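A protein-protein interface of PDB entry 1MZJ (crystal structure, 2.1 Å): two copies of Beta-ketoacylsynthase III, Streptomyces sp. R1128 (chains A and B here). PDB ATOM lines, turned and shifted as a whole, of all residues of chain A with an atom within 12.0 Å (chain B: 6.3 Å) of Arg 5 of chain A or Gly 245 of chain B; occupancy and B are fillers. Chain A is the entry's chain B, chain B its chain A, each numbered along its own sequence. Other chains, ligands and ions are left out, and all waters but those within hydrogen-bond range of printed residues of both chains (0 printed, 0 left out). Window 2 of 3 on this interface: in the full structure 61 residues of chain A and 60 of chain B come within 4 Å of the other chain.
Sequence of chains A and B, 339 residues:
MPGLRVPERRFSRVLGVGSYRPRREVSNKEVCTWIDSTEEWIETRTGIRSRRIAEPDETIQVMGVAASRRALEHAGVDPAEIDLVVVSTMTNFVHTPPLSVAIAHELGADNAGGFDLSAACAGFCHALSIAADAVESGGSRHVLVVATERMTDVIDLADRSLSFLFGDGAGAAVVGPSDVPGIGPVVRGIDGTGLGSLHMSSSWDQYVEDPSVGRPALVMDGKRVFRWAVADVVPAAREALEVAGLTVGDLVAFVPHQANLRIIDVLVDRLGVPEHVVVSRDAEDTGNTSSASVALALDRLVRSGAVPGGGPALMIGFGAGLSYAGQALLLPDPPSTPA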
ATOM      1  N   PRO A   2     -27.252  -4.362   8.044  1.00  0.00           N
ATOM      2  CA  PRO A   2     -26.569  -4.841   6.852  1.00  0.00           C
ATOM      3  C   PRO A   2     -25.132  -5.272   7.162  1.00  0.00           C
ATOM      4  O   PRO A   2     -24.164  -4.764   6.613  1.00  0.00           O
ATOM      5  CB  PRO A   2     -26.566  -3.706   5.830  1.00  0.00           C
ATOM      6  CG  PRO A   2     -27.597  -2.667   6.265  1.00  0.00           C
ATOM      7  CD  PRO A   2     -28.123  -3.262   7.657  1.00  0.00           C
ATOM      8  N   GLY A   3     -25.016  -6.219   8.113  1.00  0.00           N
ATOM      9  CA  GLY A   3     -23.786  -6.821   8.612  1.00  0.00           C
ATOM     10  C   GLY A   3     -23.659  -8.264   8.114  1.00  0.00           C
ATOM     11  O   GLY A   3     -23.005  -9.106   8.714  1.00  0.00           O
ATOM     12  N   LEU A   4     -24.458  -8.602   7.099  1.00  0.00           N
ATOM     13  CA  LEU A   4     -24.303  -9.896   6.443  1.00  0.00           C
ATOM     14  C   LEU A   4     -24.850 -11.031   7.312  1.00  0.00           C
ATOM     15  O   LEU A   4     -25.246 -10.849   8.456  1.00  0.00           O
ATOM     16  CB  LEU A   4     -22.818 -10.101   6.135  1.00  0.00           C
ATOM     17  CG  LEU A   4     -22.312  -9.168   5.033  1.00  0.00           C
ATOM     18  CD1 LEU A   4     -21.215  -9.812   4.183  1.00  0.00           C
ATOM     19  CD2 LEU A   4     -23.412  -8.741   4.060  1.00  0.00           C
ATOM     20  N   ARG A   5     -24.902 -12.234   6.712  1.00  0.00           N
ATOM     21  CA  ARG A   5     -25.375 -13.378   7.482  1.00  0.00           C
ATOM     22  C   ARG A   5     -24.214 -14.067   8.207  1.00  0.00           C
ATOM     23  O   ARG A   5     -23.084 -14.112   7.737  1.00  0.00           O
ATOM     24  CB  ARG A   5     -26.046 -14.364   6.527  1.00  0.00           C
ATOM     25  CG  ARG A   5     -26.687 -15.539   7.264  1.00  0.00           C
ATOM     26  CD  ARG A   5     -27.655 -16.317   6.367  1.00  0.00           C
ATOM     27  NE  ARG A   5     -28.842 -15.510   6.073  1.00  0.00           N
ATOM     28  CZ  ARG A   5     -29.666 -15.957   5.108  1.00  0.00           C
ATOM     29  NH1 ARG A   5     -29.393 -17.081   4.470  1.00  0.00           N
ATOM     30  NH2 ARG A   5     -30.754 -15.248   4.789  1.00  0.00           N
ATOM     31  N   VAL A   6     -24.521 -14.581   9.413  1.00  0.00           N
ATOM     32  CA  VAL A   6     -23.503 -15.304  10.167  1.00  0.00           C
ATOM     33  C   VAL A   6     -23.466 -16.784   9.781  1.00  0.00           C
ATOM     34  O   VAL A   6     -24.126 -17.632  10.369  1.00  0.00           O
ATOM     35  CB  VAL A   6     -23.821 -15.162  11.656  1.00  0.00           C
ATOM     36  CG1 VAL A   6     -22.774 -15.904  12.485  1.00  0.00           C
ATOM     37  CG2 VAL A   6     -23.821 -13.696  12.050  1.00  0.00           C
ATOM     38  N   PRO A   7     -22.687 -17.078   8.724  1.00  0.00           N
ATOM     39  CA  PRO A   7     -22.648 -18.446   8.220  1.00  0.00           C
ATOM     40  C   PRO A   7     -22.265 -19.440   9.320  1.00  0.00           C
ATOM     41  O   PRO A   7     -21.532 -19.136  10.252  1.00  0.00           O
ATOM     42  CB  PRO A   7     -21.627 -18.508   7.084  1.00  0.00           C
ATOM     43  CG  PRO A   7     -21.026 -17.118   6.905  1.00  0.00           C
ATOM     44  CD  PRO A   7     -21.508 -16.381   8.239  1.00  0.00           C
ATOM     45  N   GLU A   8     -22.827 -20.658   9.206  1.00  0.00           N
ATOM     46  CA  GLU A   8     -22.529 -21.683  10.199  1.00  0.00           C
ATOM     47  C   GLU A   8     -21.435 -22.636   9.713  1.00  0.00           C
ATOM     48  O   GLU A   8     -21.627 -23.454   8.822  1.00  0.00           O
ATOM     49  CB  GLU A   8     -23.814 -22.465  10.479  1.00  0.00           C
ATOM     50  CG  GLU A   8     -23.688 -23.945  10.113  1.00  0.00           C
ATOM     51  CD  GLU A   8     -24.982 -24.654  10.442  1.00  0.00           C
ATOM     52  OE1 GLU A   8     -25.682 -24.209  11.340  1.00  0.00           O
ATOM     53  OE2 GLU A   8     -25.280 -25.655   9.791  1.00  0.00           O
ATOM     54  N   ARG A   9     -20.238 -22.480  10.308  1.00  0.00           N
ATOM     55  CA  ARG A   9     -19.123 -23.334   9.918  1.00  0.00           C
ATOM     56  C   ARG A   9     -19.413 -24.809  10.206  1.00  0.00           C
ATOM     57  O   ARG A   9     -20.527 -25.291  10.052  1.00  0.00           O
ATOM     58  CB  ARG A   9     -17.883 -22.885  10.694  1.00  0.00           C
ATOM     59  CG  ARG A   9     -17.254 -21.622  10.106  1.00  0.00           C
ATOM     60  CD  ARG A   9     -18.300 -20.534   9.830  1.00  0.00           C
ATOM     61  NE  ARG A   9     -17.673 -19.209   9.820  1.00  0.00           N
ATOM     62  CZ  ARG A   9     -17.750 -18.497   8.681  1.00  0.00           C
ATOM     63  NH1 ARG A   9     -18.374 -18.996   7.627  1.00  0.00           N
ATOM     64  NH2 ARG A   9     -17.189 -17.286   8.618  1.00  0.00           N
ATOM     65  N   GLU A 136     -15.496 -26.025   5.480  1.00  0.00           N
ATOM     66  CA  GLU A 136     -15.633 -25.609   6.870  1.00  0.00           C
ATOM     67  C   GLU A 136     -16.304 -24.278   7.067  1.00  0.00           C
ATOM     68  O   GLU A 136     -16.788 -23.993   8.177  1.00  0.00           O
ATOM     69  CB  GLU A 136     -14.286 -25.632   7.571  1.00  0.00           C
ATOM     70  CG  GLU A 136     -13.723 -27.048   7.575  1.00  0.00           C
ATOM     71  CD  GLU A 136     -12.268 -27.105   7.952  1.00  0.00           C
ATOM     72  OE1 GLU A 136     -11.584 -28.099   7.557  1.00  0.00           O
ATOM     73  OE2 GLU A 136     -11.807 -26.168   8.631  1.00  0.00           O
ATOM     74  N   SER A 137     -16.375 -23.486   5.990  1.00  0.00           N
ATOM     75  CA  SER A 137     -17.001 -22.163   6.019  1.00  0.00           C
ATOM     76  C   SER A 137     -18.524 -22.309   5.947  1.00  0.00           C
ATOM     77  O   SER A 137     -19.287 -21.334   6.140  1.00  0.00           O
ATOM     78  CB  SER A 137     -16.560 -21.374   4.789  1.00  0.00           C
ATOM     79  OG  SER A 137     -17.322 -21.856   3.678  1.00  0.00           O
ATOM     80  N   GLY A 138     -18.979 -23.518   5.663  1.00  0.00           N
ATOM     81  CA  GLY A 138     -20.421 -23.776   5.500  1.00  0.00           C
ATOM     82  C   GLY A 138     -20.924 -23.436   4.084  1.00  0.00           C
ATOM     83  O   GLY A 138     -22.071 -23.699   3.731  1.00  0.00           O
ATOM     84  N   GLY A 139     -20.051 -22.876   3.253  1.00  0.00           N
ATOM     85  CA  GLY A 139     -20.464 -22.469   1.936  1.00  0.00           C
ATOM     86  C   GLY A 139     -20.474 -23.552   0.900  1.00  0.00           C
ATOM     87  O   GLY A 139     -21.205 -23.440  -0.093  1.00  0.00           O
ATOM     88  N   PHE B  11     -13.856 -13.059  11.514  1.00  0.00           N
ATOM     89  CA  PHE B  11     -14.632 -12.625  10.367  1.00  0.00           C
ATOM     90  C   PHE B  11     -13.653 -11.854   9.495  1.00  0.00           C
ATOM     91  O   PHE B  11     -12.590 -11.493   9.984  1.00  0.00           O
ATOM     92  CB  PHE B  11     -15.768 -11.712  10.822  1.00  0.00           C
ATOM     93  CG  PHE B  11     -16.935 -12.455  11.371  1.00  0.00           C
ATOM     94  CD1 PHE B  11     -17.543 -13.385  10.564  1.00  0.00           C
ATOM     95  CD2 PHE B  11     -17.432 -12.243  12.692  1.00  0.00           C
ATOM     96  CE1 PHE B  11     -18.645 -14.131  10.984  1.00  0.00           C
ATOM     97  CE2 PHE B  11     -18.552 -12.991  13.151  1.00  0.00           C
ATOM     98  CZ  PHE B  11     -19.163 -13.946  12.282  1.00  0.00           C
ATOM     99  N   PRO B 181     -19.081 -10.208   9.902  1.00  0.00           N
ATOM    100  CA  PRO B 181     -18.857 -10.720   8.561  1.00  0.00           C
ATOM    101  C   PRO B 181     -18.856  -9.595   7.533  1.00  0.00           C
ATOM    102  O   PRO B 181     -19.850  -8.865   7.361  1.00  0.00           O
ATOM    103  CB  PRO B 181     -19.986 -11.733   8.382  1.00  0.00           C
ATOM    104  CG  PRO B 181     -21.072 -11.184   9.193  1.00  0.00           C
ATOM    105  CD  PRO B 181     -20.331 -10.743  10.459  1.00  0.00           C
ATOM    106  N   PRO B 185     -20.788 -15.370   1.408  1.00  0.00           N
ATOM    107  CA  PRO B 185     -20.392 -16.663   0.852  1.00  0.00           C
ATOM    108  C   PRO B 185     -20.306 -16.502  -0.702  1.00  0.00           C
ATOM    109  O   PRO B 185     -21.081 -15.760  -1.291  1.00  0.00           O
ATOM    110  CB  PRO B 185     -21.566 -17.583   1.249  1.00  0.00           C
ATOM    111  CG  PRO B 185     -22.201 -16.870   2.499  1.00  0.00           C
ATOM    112  CD  PRO B 185     -22.097 -15.429   2.085  1.00  0.00           C
ATOM    113  N   ALA B 240     -26.186 -14.872  -4.818  1.00  0.00           N
ATOM    114  CA  ALA B 240     -25.127 -14.199  -4.022  1.00  0.00           C
ATOM    115  C   ALA B 240     -25.684 -13.272  -2.941  1.00  0.00           C
ATOM    116  O   ALA B 240     -25.145 -13.153  -1.827  1.00  0.00           O
ATOM    117  CB  ALA B 240     -24.239 -13.355  -4.927  1.00  0.00           C
ATOM    118  N   LEU B 241     -26.747 -12.565  -3.280  1.00  0.00           N
ATOM    119  CA  LEU B 241     -27.326 -11.649  -2.295  1.00  0.00           C
ATOM    120  C   LEU B 241     -28.002 -12.488  -1.209  1.00  0.00           C
ATOM    121  O   LEU B 241     -27.793 -12.267  -0.006  1.00  0.00           O
ATOM    122  CB  LEU B 241     -28.347 -10.742  -2.996  1.00  0.00           C
ATOM    123  CG  LEU B 241     -27.803  -9.775  -4.058  1.00  0.00           C
ATOM    124  CD1 LEU B 241     -28.993  -8.975  -4.629  1.00  0.00           C
ATOM    125  CD2 LEU B 241     -26.860  -8.742  -3.383  1.00  0.00           C
ATOM    126  N   GLU B 242     -28.812 -13.457  -1.639  1.00  0.00           N
ATOM    127  CA  GLU B 242     -29.508 -14.339  -0.684  1.00  0.00           C
ATOM    128  C   GLU B 242     -28.628 -15.073   0.326  1.00  0.00           C
ATOM    129  O   GLU B 242     -28.916 -15.044   1.525  1.00  0.00           O
ATOM    130  CB  GLU B 242     -30.350 -15.386  -1.422  1.00  0.00           C
ATOM    131  CG  GLU B 242     -31.166 -14.766  -2.501  1.00  0.00           C
ATOM    132  CD  GLU B 242     -32.184 -15.704  -3.148  1.00  0.00           C
ATOM    133  OE1 GLU B 242     -31.808 -16.619  -3.963  1.00  0.00           O
ATOM    134  OE2 GLU B 242     -33.392 -15.494  -2.849  1.00  0.00           O
ATOM    135  N   VAL B 243     -27.556 -15.729  -0.121  1.00  0.00           N
ATOM    136  CA  VAL B 243     -26.758 -16.473   0.864  1.00  0.00           C
ATOM    137  C   VAL B 243     -26.034 -15.560   1.777  1.00  0.00           C
ATOM    138  O   VAL B 243     -25.454 -16.018   2.730  1.00  0.00           O
ATOM    139  CB  VAL B 243     -25.743 -17.466   0.239  1.00  0.00           C
ATOM    140  CG1 VAL B 243     -26.500 -18.611  -0.434  1.00  0.00           C
ATOM    141  CG2 VAL B 243     -24.793 -16.716  -0.744  1.00  0.00           C
ATOM    142  N   ALA B 244     -26.061 -14.257   1.503  1.00  0.00           N
ATOM    143  CA  ALA B 244     -25.386 -13.322   2.398  1.00  0.00           C
ATOM    144  C   ALA B 244     -26.421 -12.609   3.261  1.00  0.00           C
ATOM    145  O   ALA B 244     -26.072 -11.733   4.073  1.00  0.00           O
ATOM    146  CB  ALA B 244     -24.572 -12.283   1.611  1.00  0.00           C
ATOM    147  N   GLY B 245     -27.685 -12.993   3.054  1.00  0.00           N
ATOM    148  CA  GLY B 245     -28.811 -12.405   3.779  1.00  0.00           C
ATOM    149  C   GLY B 245     -29.150 -10.990   3.321  1.00  0.00           C
ATOM    150  O   GLY B 245     -29.492 -10.162   4.150  1.00  0.00           O
ATOM    151  N   LEU B 246     -29.057 -10.714   2.021  1.00  0.00           N
ATOM    152  CA  LEU B 246     -29.331  -9.392   1.501  1.00  0.00           C
ATOM    153  C   LEU B 246     -30.320  -9.503   0.372  1.00  0.00           C
ATOM    154  O   LEU B 246     -30.457 -10.581  -0.209  1.00  0.00           O
ATOM    155  CB  LEU B 246     -28.043  -8.762   0.930  1.00  0.00           C
ATOM    156  CG  LEU B 246     -26.816  -8.544   1.829  1.00  0.00           C
ATOM    157  CD1 LEU B 246     -25.568  -8.341   0.976  1.00  0.00           C
ATOM    158  CD2 LEU B 246     -26.995  -7.325   2.745  1.00  0.00           C
ATOM    159  N   THR B 247     -31.007  -8.388   0.090  1.00  0.00           N
ATOM    160  CA  THR B 247     -31.912  -8.249  -1.076  1.00  0.00           C
ATOM    161  C   THR B 247     -31.207  -7.166  -1.966  1.00  0.00           C
ATOM    162  O   THR B 247     -30.275  -6.485  -1.496  1.00  0.00           O
ATOM    163  CB  THR B 247     -33.310  -7.668  -0.678  1.00  0.00           C
ATOM    164  OG1 THR B 247     -33.095  -6.406  -0.034  1.00  0.00           O
ATOM    165  CG2 THR B 247     -34.077  -8.619   0.301  1.00  0.00           C
ATOM    166  N   ASP B 250     -30.804  -3.318  -0.327  1.00  0.00           N
ATOM    167  CA  ASP B 250     -29.712  -2.978   0.579  1.00  0.00           C
ATOM    168  C   ASP B 250     -28.355  -2.711  -0.080  1.00  0.00           C
ATOM    169  O   ASP B 250     -27.372  -2.381   0.573  1.00  0.00           O
ATOM    170  CB  ASP B 250     -29.737  -3.968   1.745  1.00  0.00           C
ATOM    171  CG  ASP B 250     -31.167  -4.450   1.958  1.00  0.00           C
ATOM    172  OD1 ASP B 250     -31.380  -5.660   1.882  1.00  0.00           O
ATOM    173  OD2 ASP B 250     -32.042  -3.620   2.192  1.00  0.00           O
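O of Leu 241 of chain B sits at hydrogen-bond distance from N of Leu 246 of chain B.
The backbone carbonyl oxygen (O) of Ala 244 of chain B is in hydrogen-bond range of the backbone NH (N) of Arg 5 of chain A (2.9 Å).
O of Pro 181 of chain B sits close to O of Gly 3 of chain A, 3.4 Å away.
Of the printed residues of chain B, Gly 3 of chain A touches Pro 181 (2.9 Å).
Printed residues of chain B within 4 Å of Leu 4 of chain A: Pro 181, Ala 244 and Leu 246.
Of chain B, only Pro 181 (3.8 Å), Glu 242 (3.6 Å), Ala 244 (2.9 Å) and Gly 245 (3.6 Å) come within 4 Å of Arg 5 of chain A.
Glu 136 of chain A touches none of the printed residues of chain B.
Of chain A, only Gly 3, Leu 4 and Arg 5 come within 4 Å of Pro 181 of chain B.
Of the printed residues of chain A, Glu 242 of chain B touches Arg 5.
Val 243 of chain B touches none of the printed residues of chain A.
Ala 244 of chain B touches two residues of chain A.
Gly 245 of chain B touches just one residue of chain A: Arg 5.
Leu 246 of chain B touches just one residue of chain A: Leu 4 (3.8 Å).
No residue of chain A comes within 4 Å of Thr 247 of chain B.
The nearest residue of chain A that does not touch Gly 245 of chain B is Leu 4 of chain A (5.5 Å).
Of the 12 printed residues of chain B, 5 touch a printed residue of chain A.
Printed residues of chain A that touch a printed residue of chain B: Gly 3, Leu 4 and Arg 5.
Among the printed residues, 8 pairs touch across the chains.
Among the printed residues, no Asp or Glu carboxylate lies within 4 Å of a Lys or Arg side-chain nitrogen of the other chain.
No position is printed for both chains.
Of the 8 pairs that touch across the chains among the printed residues, none has its exchanged pair printed and touching as well.
Leu 4 of chain A touches Pro 181 of chain B (CG to O, 3.4 Å).
Ala 244 of chain B touches Leu 4 of chain A.
CD1 of Leu 246 of chain B touches CD2 of Leu 4 of chain A (3.8 Å).
Pro 181 of chain B touches Arg 5 of chain A.
NH1 of Arg 5 of chain A touches O of Glu 242 of chain B, at 3.6 Å.
NH2 of Arg 5 of chain A touches CA of Gly 245 of chain B (3.6 Å).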
